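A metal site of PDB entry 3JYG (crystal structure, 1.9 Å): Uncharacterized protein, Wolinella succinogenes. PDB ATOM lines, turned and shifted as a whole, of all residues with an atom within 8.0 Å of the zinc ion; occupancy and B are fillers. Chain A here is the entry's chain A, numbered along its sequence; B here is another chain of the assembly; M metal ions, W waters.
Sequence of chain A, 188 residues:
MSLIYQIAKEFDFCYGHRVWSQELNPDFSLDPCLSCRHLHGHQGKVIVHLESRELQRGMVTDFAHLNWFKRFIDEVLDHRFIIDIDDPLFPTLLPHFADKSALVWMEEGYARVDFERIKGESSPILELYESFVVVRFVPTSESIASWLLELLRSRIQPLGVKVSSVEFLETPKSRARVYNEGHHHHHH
A ring nitrogen (ND1) of His 17 lies within hydrogen-bond range of the backbone carbonyl oxygen of Pro 139 (2.7 Å).
N of His 42 sits at hydrogen-bond distance from O of Tyr 15 (3.0 Å).
O of Cys 36 lies within hydrogen-bond range of N of Val 19 (2.9 Å).
A ring nitrogen (ND1) of His 42 lies within hydrogen-bond range of the backbone carbonyl oxygen (O) of Glu 170, at 3.3 Å.
A ring nitrogen (ND1) of His 40 sits at hydrogen-bond distance from the backbone carbonyl oxygen (O) of His 38 (2.6 Å).
Residues that only touch the zinc ion: Cys 36 (3.6 Å).
Within 4 Å of the zinc ion: His 17, Cys 36, His 40 and His 42.
The zinc ion is bound by a ring nitrogen (NE2) of His 40, 2.2 Å away.
A ring nitrogen (NE2) of His 42 binds the zinc ion.
NE2 of His 17 binds the zinc ion (2.4 Å).
Water W1 is bound to the zinc ion (2.4 Å).
The zinc ion is bound by water W2, at 2.5 Å.
The zinc ion has five donor atoms within binding distance.
Water W1 bridges the side-chain carboxylate (OE2) of Glu 170 and the side-chain sulfur (SG) of Cys 36.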
ATOM      1  N   TYR A  15      -9.776   3.034  14.400  1.00  0.00           N
ATOM      2  CA  TYR A  15      -9.087   3.754  13.339  1.00  0.00           C
ATOM      3  C   TYR A  15      -8.286   2.764  12.512  1.00  0.00           C
ATOM      4  O   TYR A  15      -8.019   1.677  12.993  1.00  0.00           O
ATOM      5  CB  TYR A  15      -8.161   4.855  13.905  1.00  0.00           C
ATOM      6  CG  TYR A  15      -7.064   4.303  14.828  1.00  0.00           C
ATOM      7  CD1 TYR A  15      -7.366   3.814  16.117  1.00  0.00           C
ATOM      8  CD2 TYR A  15      -5.708   4.276  14.419  1.00  0.00           C
ATOM      9  CE1 TYR A  15      -6.384   3.309  16.960  1.00  0.00           C
ATOM     10  CE2 TYR A  15      -4.711   3.769  15.265  1.00  0.00           C
ATOM     11  CZ  TYR A  15      -5.053   3.277  16.531  1.00  0.00           C
ATOM     12  OH  TYR A  15      -4.073   2.792  17.402  1.00  0.00           O
ATOM     13  N   GLY A  16      -7.898   3.157  11.300  1.00  0.00           N
ATOM     14  CA  GLY A  16      -6.869   2.407  10.552  1.00  0.00           C
ATOM     15  C   GLY A  16      -5.546   3.185  10.589  1.00  0.00           C
ATOM     16  O   GLY A  16      -5.545   4.410  10.817  1.00  0.00           O
ATOM     17  N   HIS A  17      -4.432   2.493  10.419  1.00  0.00           N
ATOM     18  CA  HIS A  17      -3.172   3.181  10.265  1.00  0.00           C
ATOM     19  C   HIS A  17      -2.156   2.212   9.721  1.00  0.00           C
ATOM     20  O   HIS A  17      -2.470   1.022   9.475  1.00  0.00           O
ATOM     21  CB  HIS A  17      -2.708   3.847  11.604  1.00  0.00           C
ATOM     22  CG  HIS A  17      -1.996   2.928  12.569  1.00  0.00           C
ATOM     23  ND1 HIS A  17      -1.045   3.386  13.454  1.00  0.00           N
ATOM     24  CD2 HIS A  17      -2.104   1.596  12.798  1.00  0.00           C
ATOM     25  CE1 HIS A  17      -0.598   2.386  14.188  1.00  0.00           C
ATOM     26  NE2 HIS A  17      -1.226   1.284  13.800  1.00  0.00           N
ATOM     27  N   ARG A  18      -0.950   2.734   9.518  1.00  0.00           N
ATOM     28  CA  ARG A  18       0.223   1.899   9.412  1.00  0.00           C
ATOM     29  C   ARG A  18       1.411   2.681   9.982  1.00  0.00           C
ATOM     30  O   ARG A  18       1.428   3.912   9.966  1.00  0.00           O
ATOM     31  CB  ARG A  18       0.453   1.462   7.946  1.00  0.00           C
ATOM     32  CG  ARG A  18       1.221   2.451   7.098  1.00  0.00           C
ATOM     33  CD  ARG A  18       1.490   1.881   5.694  1.00  0.00           C
ATOM     34  NE  ARG A  18       2.516   2.660   4.985  1.00  0.00           N
ATOM     35  CZ  ARG A  18       3.649   2.153   4.492  1.00  0.00           C
ATOM     36  NH1 ARG A  18       3.954   0.845   4.622  1.00  0.00           N
ATOM     37  NH2 ARG A  18       4.483   2.962   3.850  1.00  0.00           N
ATOM     38  N   VAL A  19       2.390   1.935  10.478  1.00  0.00           N
ATOM     39  CA  VAL A  19       3.614   2.488  11.043  1.00  0.00           C
ATOM     40  C   VAL A  19       4.681   2.217  10.013  1.00  0.00           C
ATOM     41  O   VAL A  19       5.221   1.135   9.968  1.00  0.00           O
ATOM     42  CB  VAL A  19       3.987   1.755  12.342  1.00  0.00           C
ATOM     43  CG1 VAL A  19       5.234   2.381  12.993  1.00  0.00           C
ATOM     44  CG2 VAL A  19       2.793   1.801  13.314  1.00  0.00           C
ATOM     45  N   SER A  35       5.235  -6.401  10.085  1.00  0.00           N
ATOM     46  CA  SER A  35       3.785  -6.431   9.957  1.00  0.00           C
ATOM     47  C   SER A  35       3.066  -5.099  10.248  1.00  0.00           C
ATOM     48  O   SER A  35       2.011  -4.832   9.697  1.00  0.00           O
ATOM     49  CB  SER A  35       3.237  -7.595  10.837  1.00  0.00           C
ATOM     50  OG  SER A  35       3.165  -7.238  12.219  1.00  0.00           O
ATOM     51  N   CYS A  36       3.654  -4.257  11.103  1.00  0.00           N
ATOM     52  CA  CYS A  36       3.078  -2.955  11.422  1.00  0.00           C
ATOM     53  C   CYS A  36       3.159  -1.982  10.209  1.00  0.00           C
ATOM     54  O   CYS A  36       2.401  -0.984  10.144  1.00  0.00           O
ATOM     55  CB  CYS A  36       3.764  -2.366  12.653  1.00  0.00           C
ATOM     56  SG  CYS A  36       2.724  -1.660  13.972  1.00  0.00           S
ATOM     57  N   ARG A  37       4.041  -2.292   9.225  1.00  0.00           N
ATOM     58  CA  ARG A  37       4.056  -1.521   7.957  1.00  0.00           C
ATOM     59  C   ARG A  37       2.797  -1.819   7.099  1.00  0.00           C
ATOM     60  O   ARG A  37       2.517  -1.104   6.114  1.00  0.00           O
ATOM     61  CB  ARG A  37       5.356  -1.732   7.119  1.00  0.00           C
ATOM     62  CG  ARG A  37       6.625  -1.209   7.795  1.00  0.00           C
ATOM     63  CD  ARG A  37       7.845  -1.331   6.880  1.00  0.00           C
ATOM     64  NE  ARG A  37       9.088  -0.932   7.550  1.00  0.00           N
ATOM     65  CZ  ARG A  37      10.165  -0.410   6.950  1.00  0.00           C
ATOM     66  NH1 ARG A  37      10.188  -0.233   5.631  1.00  0.00           N
ATOM     67  NH2 ARG A  37      11.228  -0.070   7.661  1.00  0.00           N
ATOM     68  N   HIS A  38       2.068  -2.877   7.431  1.00  0.00           N
ATOM     69  CA  HIS A  38       0.811  -3.161   6.677  1.00  0.00           C
ATOM     70  C   HIS A  38      -0.288  -2.167   7.010  1.00  0.00           C
ATOM     71  O   HIS A  38      -0.362  -1.690   8.150  1.00  0.00           O
ATOM     72  CB  HIS A  38       0.339  -4.583   6.930  1.00  0.00           C
ATOM     73  CG  HIS A  38       1.318  -5.615   6.442  1.00  0.00           C
ATOM     74  ND1 HIS A  38       1.413  -6.875   6.980  1.00  0.00           N
ATOM     75  CD2 HIS A  38       2.262  -5.540   5.466  1.00  0.00           C
ATOM     76  CE1 HIS A  38       2.362  -7.551   6.356  1.00  0.00           C
ATOM     77  NE2 HIS A  38       2.906  -6.761   5.444  1.00  0.00           N
ATOM     78  N   LEU A  39      -1.116  -1.830   6.031  1.00  0.00           N
ATOM     79  CA  LEU A  39      -2.389  -1.151   6.317  1.00  0.00           C
ATOM     80  C   LEU A  39      -3.163  -2.054   7.259  1.00  0.00           C
ATOM     81  O   LEU A  39      -3.392  -3.246   6.958  1.00  0.00           O
ATOM     82  CB  LEU A  39      -3.223  -0.962   5.044  1.00  0.00           C
ATOM     83  CG  LEU A  39      -2.657  -0.216   3.817  1.00  0.00           C
ATOM     84  CD1 LEU A  39      -3.782   0.143   2.808  1.00  0.00           C
ATOM     85  CD2 LEU A  39      -1.869   0.999   4.232  1.00  0.00           C
ATOM     86  N   HIS A  40      -3.518  -1.522   8.418  1.00  0.00           N
ATOM     87  CA  HIS A  40      -4.345  -2.277   9.386  1.00  0.00           C
ATOM     88  C   HIS A  40      -5.143  -1.303  10.252  1.00  0.00           C
ATOM     89  O   HIS A  40      -5.393  -0.160   9.839  1.00  0.00           O
ATOM     90  CB  HIS A  40      -3.476  -3.260  10.218  1.00  0.00           C
ATOM     91  CG  HIS A  40      -2.435  -2.591  11.047  1.00  0.00           C
ATOM     92  ND1 HIS A  40      -1.241  -2.141  10.531  1.00  0.00           N
ATOM     93  CD2 HIS A  40      -2.392  -2.303  12.382  1.00  0.00           C
ATOM     94  CE1 HIS A  40      -0.519  -1.593  11.495  1.00  0.00           C
ATOM     95  NE2 HIS A  40      -1.184  -1.710  12.641  1.00  0.00           N
ATOM     96  N   GLY A  41      -5.565  -1.743  11.417  1.00  0.00           N
ATOM     97  CA  GLY A  41      -6.361  -0.912  12.299  1.00  0.00           C
ATOM     98  C   GLY A  41      -6.378  -1.470  13.707  1.00  0.00           C
ATOM     99  O   GLY A  41      -5.759  -2.528  13.965  1.00  0.00           O
ATOM    100  N   HIS A  42      -7.111  -0.766  14.573  1.00  0.00           N
ATOM    101  CA  HIS A  42      -7.130  -0.994  16.007  1.00  0.00           C
ATOM    102  C   HIS A  42      -8.366  -0.434  16.645  1.00  0.00           C
ATOM    103  O   HIS A  42      -8.957   0.501  16.122  1.00  0.00           O
ATOM    104  CB  HIS A  42      -5.975  -0.235  16.647  1.00  0.00           C
ATOM    105  CG  HIS A  42      -4.670  -0.802  16.299  1.00  0.00           C
ATOM    106  ND1 HIS A  42      -4.308  -2.100  16.612  1.00  0.00           N
ATOM    107  CD2 HIS A  42      -3.630  -0.273  15.605  1.00  0.00           C
ATOM    108  CE1 HIS A  42      -3.098  -2.329  16.148  1.00  0.00           C
ATOM    109  NE2 HIS A  42      -2.665  -1.231  15.554  1.00  0.00           N
ATOM    110  N   PRO A 139       2.265   7.428  13.160  1.00  0.00           N
ATOM    111  CA  PRO A 139       1.189   7.279  14.184  1.00  0.00           C
ATOM    112  C   PRO A 139       1.296   5.991  15.022  1.00  0.00           C
ATOM    113  O   PRO A 139       0.373   5.147  14.983  1.00  0.00           O
ATOM    114  CB  PRO A 139      -0.110   7.307  13.353  1.00  0.00           C
ATOM    115  CG  PRO A 139       0.345   6.758  11.952  1.00  0.00           C
ATOM    116  CD  PRO A 139       1.799   7.220  11.772  1.00  0.00           C
ATOM    117  N   THR A 140       2.398   5.854  15.762  1.00  0.00           N
ATOM    118  CA  THR A 140       2.577   4.810  16.759  1.00  0.00           C
ATOM    119  C   THR A 140       1.708   5.127  17.967  1.00  0.00           C
ATOM    120  O   THR A 140       1.292   6.281  18.136  1.00  0.00           O
ATOM    121  CB  THR A 140       4.024   4.775  17.267  1.00  0.00           C
ATOM    122  OG1 THR A 140       4.402   6.082  17.714  1.00  0.00           O
ATOM    123  CG2 THR A 140       4.989   4.384  16.135  1.00  0.00           C
ATOM    124  N   SER A 141       1.462   4.131  18.833  1.00  0.00           N
ATOM    125  CA  SER A 141       0.827   4.381  20.126  1.00  0.00           C
ATOM    126  C   SER A 141       1.477   5.474  20.921  1.00  0.00           C
ATOM    127  O   SER A 141       0.793   6.313  21.454  1.00  0.00           O
ATOM    128  CB  SER A 141       0.844   3.110  20.956  1.00  0.00           C
ATOM    129  OG  SER A 141       0.014   2.196  20.251  1.00  0.00           O
ATOM    130  N   GLU A 170      -3.173   0.476  22.334  1.00  0.00           N
ATOM    131  CA  GLU A 170      -3.207   0.086  20.945  1.00  0.00           C
ATOM    132  C   GLU A 170      -4.024  -1.242  20.821  1.00  0.00           C
ATOM    133  O   GLU A 170      -4.725  -1.485  19.826  1.00  0.00           O
ATOM    134  CB  GLU A 170      -1.763  -0.178  20.521  1.00  0.00           C
ATOM    135  CG  GLU A 170      -1.589  -0.618  19.115  1.00  0.00           C
ATOM    136  CD  GLU A 170      -0.172  -1.098  18.893  1.00  0.00           C
ATOM    137  OE1 GLU A 170       0.773  -0.290  19.144  1.00  0.00           O
ATOM    138  OE2 GLU A 170      -0.021  -2.265  18.474  1.00  0.00           O
ATOM    139  N   THR A 171      -3.839  -2.114  21.824  1.00  0.00           N
ATOM    140  CA  THR A 171      -4.584  -3.364  21.943  1.00  0.00           C
ATOM    141  C   THR A 171      -4.928  -3.578  23.436  1.00  0.00           C
ATOM    142  O   THR A 171      -4.413  -2.849  24.308  1.00  0.00           O
ATOM    143  CB  THR A 171      -3.793  -4.577  21.374  1.00  0.00           C
ATOM    144  OG1 THR A 171      -2.733  -4.960  22.258  1.00  0.00           O
ATOM    145  CG2 THR A 171      -3.237  -4.318  19.953  1.00  0.00           C
ATOM    146  N   PHE B  63       6.987  -3.270  20.350  1.00  0.00           N
ATOM    147  CA  PHE B  63       6.309  -4.273  21.173  1.00  0.00           C
ATOM    148  C   PHE B  63       6.815  -5.672  20.868  1.00  0.00           C
ATOM    149  O   PHE B  63       6.908  -6.527  21.764  1.00  0.00           O
ATOM    150  CB  PHE B  63       4.772  -4.214  21.009  1.00  0.00           C
ATOM    151  CG  PHE B  63       4.109  -3.068  21.787  1.00  0.00           C
ATOM    152  CD1 PHE B  63       4.149  -3.024  23.189  1.00  0.00           C
ATOM    153  CD2 PHE B  63       3.437  -2.036  21.101  1.00  0.00           C
ATOM    154  CE1 PHE B  63       3.544  -1.989  23.888  1.00  0.00           C
ATOM    155  CE2 PHE B  63       2.836  -0.971  21.800  1.00  0.00           C
ATOM    156  CZ  PHE B  63       2.894  -0.936  23.182  1.00  0.00           C
HETATM  157 ZN    ZN M   1      -0.722  -0.878  14.572  1.00  0.00          ZN
HETATM  158  O   HOH W   1       0.128  -2.896  15.509  1.00  0.00           O
HETATM  159  O   HOH W   2       0.298   0.300  16.523  1.00  0.00           O
